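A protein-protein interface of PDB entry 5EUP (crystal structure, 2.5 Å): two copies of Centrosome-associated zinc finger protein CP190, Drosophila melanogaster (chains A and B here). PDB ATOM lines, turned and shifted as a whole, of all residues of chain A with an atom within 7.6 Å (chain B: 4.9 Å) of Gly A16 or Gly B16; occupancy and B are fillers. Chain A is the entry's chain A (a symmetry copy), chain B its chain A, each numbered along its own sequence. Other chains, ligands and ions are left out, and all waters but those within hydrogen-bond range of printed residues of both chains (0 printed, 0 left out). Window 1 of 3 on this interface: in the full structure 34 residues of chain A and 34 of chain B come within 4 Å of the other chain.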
ATOM      1  N   LYS A  11      21.889   2.720  32.927  1.00  0.00           N
ATOM      2  CA  LYS A  11      22.545   2.968  31.646  1.00  0.00           C
ATOM      3  C   LYS A  11      23.081   1.705  30.980  1.00  0.00           C
ATOM      4  O   LYS A  11      23.229   0.661  31.613  1.00  0.00           O
ATOM      5  CB  LYS A  11      23.683   3.976  31.812  1.00  0.00           C
ATOM      6  CG  LYS A  11      24.834   3.474  32.665  1.00  0.00           C
ATOM      7  CD  LYS A  11      26.104   4.262  32.392  1.00  0.00           C
ATOM      8  CE  LYS A  11      26.547   4.098  30.946  1.00  0.00           C
ATOM      9  NZ  LYS A  11      27.813   4.829  30.661  1.00  0.00           N
ATOM     10  N   VAL A  12      23.368   1.824  29.687  1.00  0.00           N
ATOM     11  CA  VAL A  12      24.002   0.758  28.925  1.00  0.00           C
ATOM     12  C   VAL A  12      25.387   1.218  28.489  1.00  0.00           C
ATOM     13  O   VAL A  12      25.517   2.107  27.648  1.00  0.00           O
ATOM     14  CB  VAL A  12      23.181   0.392  27.676  1.00  0.00           C
ATOM     15  CG1 VAL A  12      23.915  -0.649  26.845  1.00  0.00           C
ATOM     16  CG2 VAL A  12      21.800  -0.109  28.074  1.00  0.00           C
ATOM     17  N   ASP A  13      26.420   0.617  29.072  1.00  0.00           N
ATOM     18  CA  ASP A  13      27.797   0.999  28.767  1.00  0.00           C
ATOM     19  C   ASP A  13      28.187   0.637  27.339  1.00  0.00           C
ATOM     20  O   ASP A  13      27.544  -0.199  26.703  1.00  0.00           O
ATOM     21  CB  ASP A  13      28.767   0.366  29.765  1.00  0.00           C
ATOM     22  CG  ASP A  13      28.669   0.986  31.145  1.00  0.00           C
ATOM     23  OD1 ASP A  13      29.408   1.957  31.414  1.00  0.00           O
ATOM     24  OD2 ASP A  13      27.853   0.505  31.958  1.00  0.00           O
ATOM     25  N   ASN A  14      29.244   1.280  26.848  1.00  0.00           N
ATOM     26  CA  ASN A  14      29.700   1.122  25.468  1.00  0.00           C
ATOM     27  C   ASN A  14      28.615   1.458  24.448  1.00  0.00           C
ATOM     28  O   ASN A  14      28.578   0.885  23.359  1.00  0.00           O
ATOM     29  CB  ASN A  14      30.236  -0.293  25.222  1.00  0.00           C
ATOM     30  CG  ASN A  14      31.309  -0.689  26.215  1.00  0.00           C
ATOM     31  OD1 ASN A  14      31.999   0.163  26.775  1.00  0.00           O
ATOM     32  ND2 ASN A  14      31.458  -1.990  26.438  1.00  0.00           N
ATOM     33  N   TRP A  15      27.736   2.387  24.809  1.00  0.00           N
ATOM     34  CA  TRP A  15      26.649   2.798  23.930  1.00  0.00           C
ATOM     35  C   TRP A  15      27.162   3.699  22.814  1.00  0.00           C
ATOM     36  O   TRP A  15      26.638   3.677  21.701  1.00  0.00           O
ATOM     37  CB  TRP A  15      25.552   3.513  24.725  1.00  0.00           C
ATOM     38  CG  TRP A  15      24.484   4.111  23.864  1.00  0.00           C
ATOM     39  CD1 TRP A  15      24.321   5.431  23.558  1.00  0.00           C
ATOM     40  CD2 TRP A  15      23.437   3.408  23.184  1.00  0.00           C
ATOM     41  NE1 TRP A  15      23.231   5.593  22.734  1.00  0.00           N
ATOM     42  CE2 TRP A  15      22.673   4.366  22.489  1.00  0.00           C
ATOM     43  CE3 TRP A  15      23.070   2.060  23.096  1.00  0.00           C
ATOM     44  CZ2 TRP A  15      21.565   4.022  21.718  1.00  0.00           C
ATOM     45  CZ3 TRP A  15      21.970   1.720  22.331  1.00  0.00           C
ATOM     46  CH2 TRP A  15      21.231   2.698  21.651  1.00  0.00           C
ATOM     47  N   GLY A  16      28.188   4.487  23.123  1.00  0.00           N
ATOM     48  CA  GLY A  16      28.788   5.386  22.154  1.00  0.00           C
ATOM     49  C   GLY A  16      29.325   4.643  20.948  1.00  0.00           C
ATOM     50  O   GLY A  16      28.983   4.956  19.807  1.00  0.00           O
ATOM     51  N   VAL A  17      30.166   3.649  21.209  1.00  0.00           N
ATOM     52  CA  VAL A  17      30.738   2.829  20.150  1.00  0.00           C
ATOM     53  C   VAL A  17      29.658   1.988  19.468  1.00  0.00           C
ATOM     54  O   VAL A  17      29.705   1.770  18.256  1.00  0.00           O
ATOM     55  CB  VAL A  17      31.886   1.939  20.685  1.00  0.00           C
ATOM     56  CG1 VAL A  17      31.439   1.150  21.903  1.00  0.00           C
ATOM     57  CG2 VAL A  17      32.417   1.015  19.593  1.00  0.00           C
ATOM     58  N   PHE A  18      28.677   1.534  20.244  1.00  0.00           N
ATOM     59  CA  PHE A  18      27.573   0.744  19.705  1.00  0.00           C
ATOM     60  C   PHE A  18      26.727   1.577  18.756  1.00  0.00           C
ATOM     61  O   PHE A  18      26.360   1.118  17.676  1.00  0.00           O
ATOM     62  CB  PHE A  18      26.699   0.193  20.833  1.00  0.00           C
ATOM     63  CG  PHE A  18      25.486  -0.553  20.353  1.00  0.00           C
ATOM     64  CD1 PHE A  18      25.594  -1.862  19.909  1.00  0.00           C
ATOM     65  CD2 PHE A  18      24.240   0.050  20.350  1.00  0.00           C
ATOM     66  CE1 PHE A  18      24.481  -2.553  19.467  1.00  0.00           C
ATOM     67  CE2 PHE A  18      23.122  -0.635  19.909  1.00  0.00           C
ATOM     68  CZ  PHE A  18      23.242  -1.939  19.468  1.00  0.00           C
ATOM     69  N   PHE A  19      26.411   2.800  19.165  1.00  0.00           N
ATOM     70  CA  PHE A  19      25.645   3.706  18.319  1.00  0.00           C
ATOM     71  C   PHE A  19      26.457   4.107  17.095  1.00  0.00           C
ATOM     72  O   PHE A  19      25.919   4.239  15.995  1.00  0.00           O
ATOM     73  CB  PHE A  19      25.223   4.951  19.102  1.00  0.00           C
ATOM     74  CG  PHE A  19      24.598   6.017  18.252  1.00  0.00           C
ATOM     75  CD1 PHE A  19      23.271   5.922  17.866  1.00  0.00           C
ATOM     76  CD2 PHE A  19      25.335   7.114  17.837  1.00  0.00           C
ATOM     77  CE1 PHE A  19      22.692   6.899  17.083  1.00  0.00           C
ATOM     78  CE2 PHE A  19      24.762   8.094  17.053  1.00  0.00           C
ATOM     79  CZ  PHE A  19      23.438   7.987  16.677  1.00  0.00           C
ATOM     80  N   LEU A  20      27.757   4.298  17.297  1.00  0.00           N
ATOM     81  CA  LEU A  20      28.648   4.697  16.216  1.00  0.00           C
ATOM     82  C   LEU A  20      28.786   3.588  15.178  1.00  0.00           C
ATOM     83  O   LEU A  20      28.844   3.858  13.979  1.00  0.00           O
ATOM     84  CB  LEU A  20      30.021   5.081  16.766  1.00  0.00           C
ATOM     85  CG  LEU A  20      31.027   5.648  15.762  1.00  0.00           C
ATOM     86  CD1 LEU A  20      30.560   6.995  15.225  1.00  0.00           C
ATOM     87  CD2 LEU A  20      32.407   5.764  16.391  1.00  0.00           C
ATOM     88  N   GLN A  21      28.832   2.341  15.642  1.00  0.00           N
ATOM     89  CA  GLN A  21      28.963   1.202  14.741  1.00  0.00           C
ATOM     90  C   GLN A  21      27.694   1.019  13.915  1.00  0.00           C
ATOM     91  O   GLN A  21      27.727   0.433  12.833  1.00  0.00           O
ATOM     92  CB  GLN A  21      29.293  -0.080  15.514  1.00  0.00           C
ATOM     93  CG  GLN A  21      28.081  -0.868  15.985  1.00  0.00           C
ATOM     94  CD  GLN A  21      28.447  -1.996  16.927  1.00  0.00           C
ATOM     95  OE1 GLN A  21      29.585  -2.096  17.384  1.00  0.00           O
ATOM     96  NE2 GLN A  21      27.478  -2.855  17.225  1.00  0.00           N
ATOM     97  N   LYS A  22      26.575   1.526  14.425  1.00  0.00           N
ATOM     98  CA  LYS A  22      25.317   1.465  13.695  1.00  0.00           C
ATOM     99  C   LYS A  22      25.340   2.431  12.514  1.00  0.00           C
ATOM    100  O   LYS A  22      24.910   2.087  11.414  1.00  0.00           O
ATOM    101  CB  LYS A  22      24.133   1.770  14.615  1.00  0.00           C
ATOM    102  CG  LYS A  22      23.925   0.751  15.727  1.00  0.00           C
ATOM    103  CD  LYS A  22      23.650  -0.640  15.172  1.00  0.00           C
ATOM    104  CE  LYS A  22      22.366  -0.671  14.358  1.00  0.00           C
ATOM    105  NZ  LYS A  22      22.072  -2.031  13.824  1.00  0.00           N
ATOM    106  N   THR A  93      34.440   6.042  12.538  1.00  0.00           N
ATOM    107  CA  THR A  93      35.128   5.020  13.321  1.00  0.00           C
ATOM    108  C   THR A  93      35.983   5.592  14.448  1.00  0.00           C
ATOM    109  O   THR A  93      36.049   5.022  15.536  1.00  0.00           O
ATOM    110  CB  THR A  93      36.026   4.136  12.428  1.00  0.00           C
ATOM    111  OG1 THR A  93      37.045   4.943  11.822  1.00  0.00           O
ATOM    112  CG2 THR A  93      35.203   3.464  11.341  1.00  0.00           C
ATOM    113  N   GLY A  94      36.642   6.715  14.185  1.00  0.00           N
ATOM    114  CA  GLY A  94      37.589   7.276  15.130  1.00  0.00           C
ATOM    115  C   GLY A  94      38.991   6.806  14.799  1.00  0.00           C
ATOM    116  O   GLY A  94      39.945   7.087  15.524  1.00  0.00           O
ATOM    117  N   ASN B  14      37.840   6.981  22.904  1.00  0.00           N
ATOM    118  CA  ASN B  14      36.637   7.650  23.394  1.00  0.00           C
ATOM    119  C   ASN B  14      35.968   8.514  22.327  1.00  0.00           C
ATOM    120  O   ASN B  14      35.353   9.533  22.639  1.00  0.00           O
ATOM    121  CB  ASN B  14      36.940   8.491  24.639  1.00  0.00           C
ATOM    122  CG  ASN B  14      37.618   7.689  25.731  1.00  0.00           C
ATOM    123  OD1 ASN B  14      37.464   6.470  25.809  1.00  0.00           O
ATOM    124  ND2 ASN B  14      38.374   8.371  26.584  1.00  0.00           N
ATOM    125  N   TRP B  15      36.095   8.099  21.071  1.00  0.00           N
ATOM    126  CA  TRP B  15      35.509   8.834  19.957  1.00  0.00           C
ATOM    127  C   TRP B  15      34.003   8.612  19.892  1.00  0.00           C
ATOM    128  O   TRP B  15      33.256   9.504  19.492  1.00  0.00           O
ATOM    129  CB  TRP B  15      36.162   8.423  18.635  1.00  0.00           C
ATOM    130  CG  TRP B  15      35.496   9.012  17.431  1.00  0.00           C
ATOM    131  CD1 TRP B  15      34.668   8.370  16.557  1.00  0.00           C
ATOM    132  CD2 TRP B  15      35.589  10.367  16.976  1.00  0.00           C
ATOM    133  NE1 TRP B  15      34.245   9.242  15.580  1.00  0.00           N
ATOM    134  CE2 TRP B  15      34.796  10.475  15.817  1.00  0.00           C
ATOM    135  CE3 TRP B  15      36.269  11.500  17.436  1.00  0.00           C
ATOM    136  CZ2 TRP B  15      34.663  11.668  15.111  1.00  0.00           C
ATOM    137  CZ3 TRP B  15      36.136  12.684  16.734  1.00  0.00           C
ATOM    138  CH2 TRP B  15      35.339  12.759  15.584  1.00  0.00           C
ATOM    139  N   GLY B  16      33.569   7.418  20.288  1.00  0.00           N
ATOM    140  CA  GLY B  16      32.159   7.074  20.293  1.00  0.00           C
ATOM    141  C   GLY B  16      31.352   8.002  21.177  1.00  0.00           C
ATOM    142  O   GLY B  16      30.367   8.597  20.738  1.00  0.00           O
ATOM    143  N   VAL B  17      31.780   8.128  22.427  1.00  0.00           N
ATOM    144  CA  VAL B  17      31.120   9.008  23.381  1.00  0.00           C
ATOM    145  C   VAL B  17      31.288  10.474  22.977  1.00  0.00           C
ATOM    146  O   VAL B  17      30.377  11.283  23.161  1.00  0.00           O
ATOM    147  CB  VAL B  17      31.631   8.762  24.822  1.00  0.00           C
ATOM    148  CG1 VAL B  17      33.147   8.819  24.876  1.00  0.00           C
ATOM    149  CG2 VAL B  17      31.006   9.751  25.801  1.00  0.00           C
ATOM    150  N   PHE B  18      32.445  10.807  22.410  1.00  0.00           N
ATOM    151  CA  PHE B  18      32.713  12.168  21.956  1.00  0.00           C
ATOM    152  C   PHE B  18      31.795  12.544  20.803  1.00  0.00           C
ATOM    153  O   PHE B  18      31.234  13.637  20.779  1.00  0.00           O
ATOM    154  CB  PHE B  18      34.173  12.318  21.525  1.00  0.00           C
ATOM    155  CG  PHE B  18      34.504  13.669  20.954  1.00  0.00           C
ATOM    156  CD1 PHE B  18      34.725  14.752  21.789  1.00  0.00           C
ATOM    157  CD2 PHE B  18      34.597  13.855  19.585  1.00  0.00           C
ATOM    158  CE1 PHE B  18      35.030  15.996  21.270  1.00  0.00           C
ATOM    159  CE2 PHE B  18      34.902  15.096  19.057  1.00  0.00           C
ATOM    160  CZ  PHE B  18      35.120  16.168  19.901  1.00  0.00           C
ATOM    161  N   PHE B  19      31.648  11.636  19.845  1.00  0.00           N
ATOM    162  CA  PHE B  19      30.757  11.866  18.716  1.00  0.00           C
ATOM    163  C   PHE B  19      29.307  11.900  19.182  1.00  0.00           C
ATOM    164  O   PHE B  19      28.502  12.688  18.683  1.00  0.00           O
ATOM    165  CB  PHE B  19      30.941  10.782  17.651  1.00  0.00           C
ATOM    166  CG  PHE B  19      29.925  10.839  16.548  1.00  0.00           C
ATOM    167  CD1 PHE B  19      30.059  11.751  15.514  1.00  0.00           C
ATOM    168  CD2 PHE B  19      28.837   9.983  16.545  1.00  0.00           C
ATOM    169  CE1 PHE B  19      29.127  11.807  14.498  1.00  0.00           C
ATOM    170  CE2 PHE B  19      27.901  10.035  15.532  1.00  0.00           C
ATOM    171  CZ  PHE B  19      28.047  10.948  14.507  1.00  0.00           C
ATOM    172  N   LEU B  20      28.984  11.042  20.143  1.00  0.00           N
ATOM    173  CA  LEU B  20      27.630  10.960  20.672  1.00  0.00           C
ATOM    174  C   LEU B  20      27.256  12.229  21.430  1.00  0.00           C
ATOM    175  O   LEU B  20      26.121  12.696  21.348  1.00  0.00           O
ATOM    176  CB  LEU B  20      27.480   9.738  21.579  1.00  0.00           C
ATOM    177  CG  LEU B  20      26.073   9.444  22.106  1.00  0.00           C
ATOM    178  CD1 LEU B  20      25.135   9.060  20.970  1.00  0.00           C
ATOM    179  CD2 LEU B  20      26.114   8.357  23.168  1.00  0.00           C
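Trp A15 touches Leu B20.
CA of Gly B16 touches C of Gly A16 (3.8 Å).
Phe B19 touches Phe A19 (CE2 to CE2, 3.99 Å).
Leu B20 touches Phe A19 (CD1 to CD2, 3.7 Å).
Leu A20 touches Trp B15.
Leu A20 touches Phe B19 (CD1 to CD2, 3.7 Å).
Thr A93 touches Trp B15.
Gly A94 touches Trp B15.
Gly A16 touches just one residue of chain B: Gly B16.
Gly B16 touches just one residue of chain A: Gly A16 (3.8 Å).
Printed residues of chain A within 4 Å of Phe B19: Phe A19 (3.99 Å) and Leu A20 (3.7 Å).
Of the printed residues of chain B, Gly A94 touches Trp B15.
Val A12 touches none of the printed residues of chain B.
Lys A11 touches none of the printed residues of chain B.
The nearest residue of chain B that does not touch Gly A16 is Val B17 (4.1 Å).
The nearest residue of chain A that does not touch Gly B16 is Val A17 (4.1 Å).
Hydrophobic or aromatic side chains of chain B that line the printed part of chain A: Trp B15, Phe B19 and Leu B20.
Along chain B the printed residues that touch a printed residue of chain A span positions 15 to 20.
Of the 14 printed residues of chain A, 6 touch a printed residue of chain B.
Among the printed residues, 8 pairs touch across the chains.
Trp A15 touches Leu B20, and with the chains exchanged Leu A20 touches Trp B15.
Gly B16 touches its own counterpart, Gly A16.
Phe A19 touches its own counterpart, Phe B19.
Phe A19 touches Leu B20, and with the chains exchanged Leu A20 touches Phe B19.
Positions printed for both chains: 14, 15, 16, 17, 18, 19 and 20.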
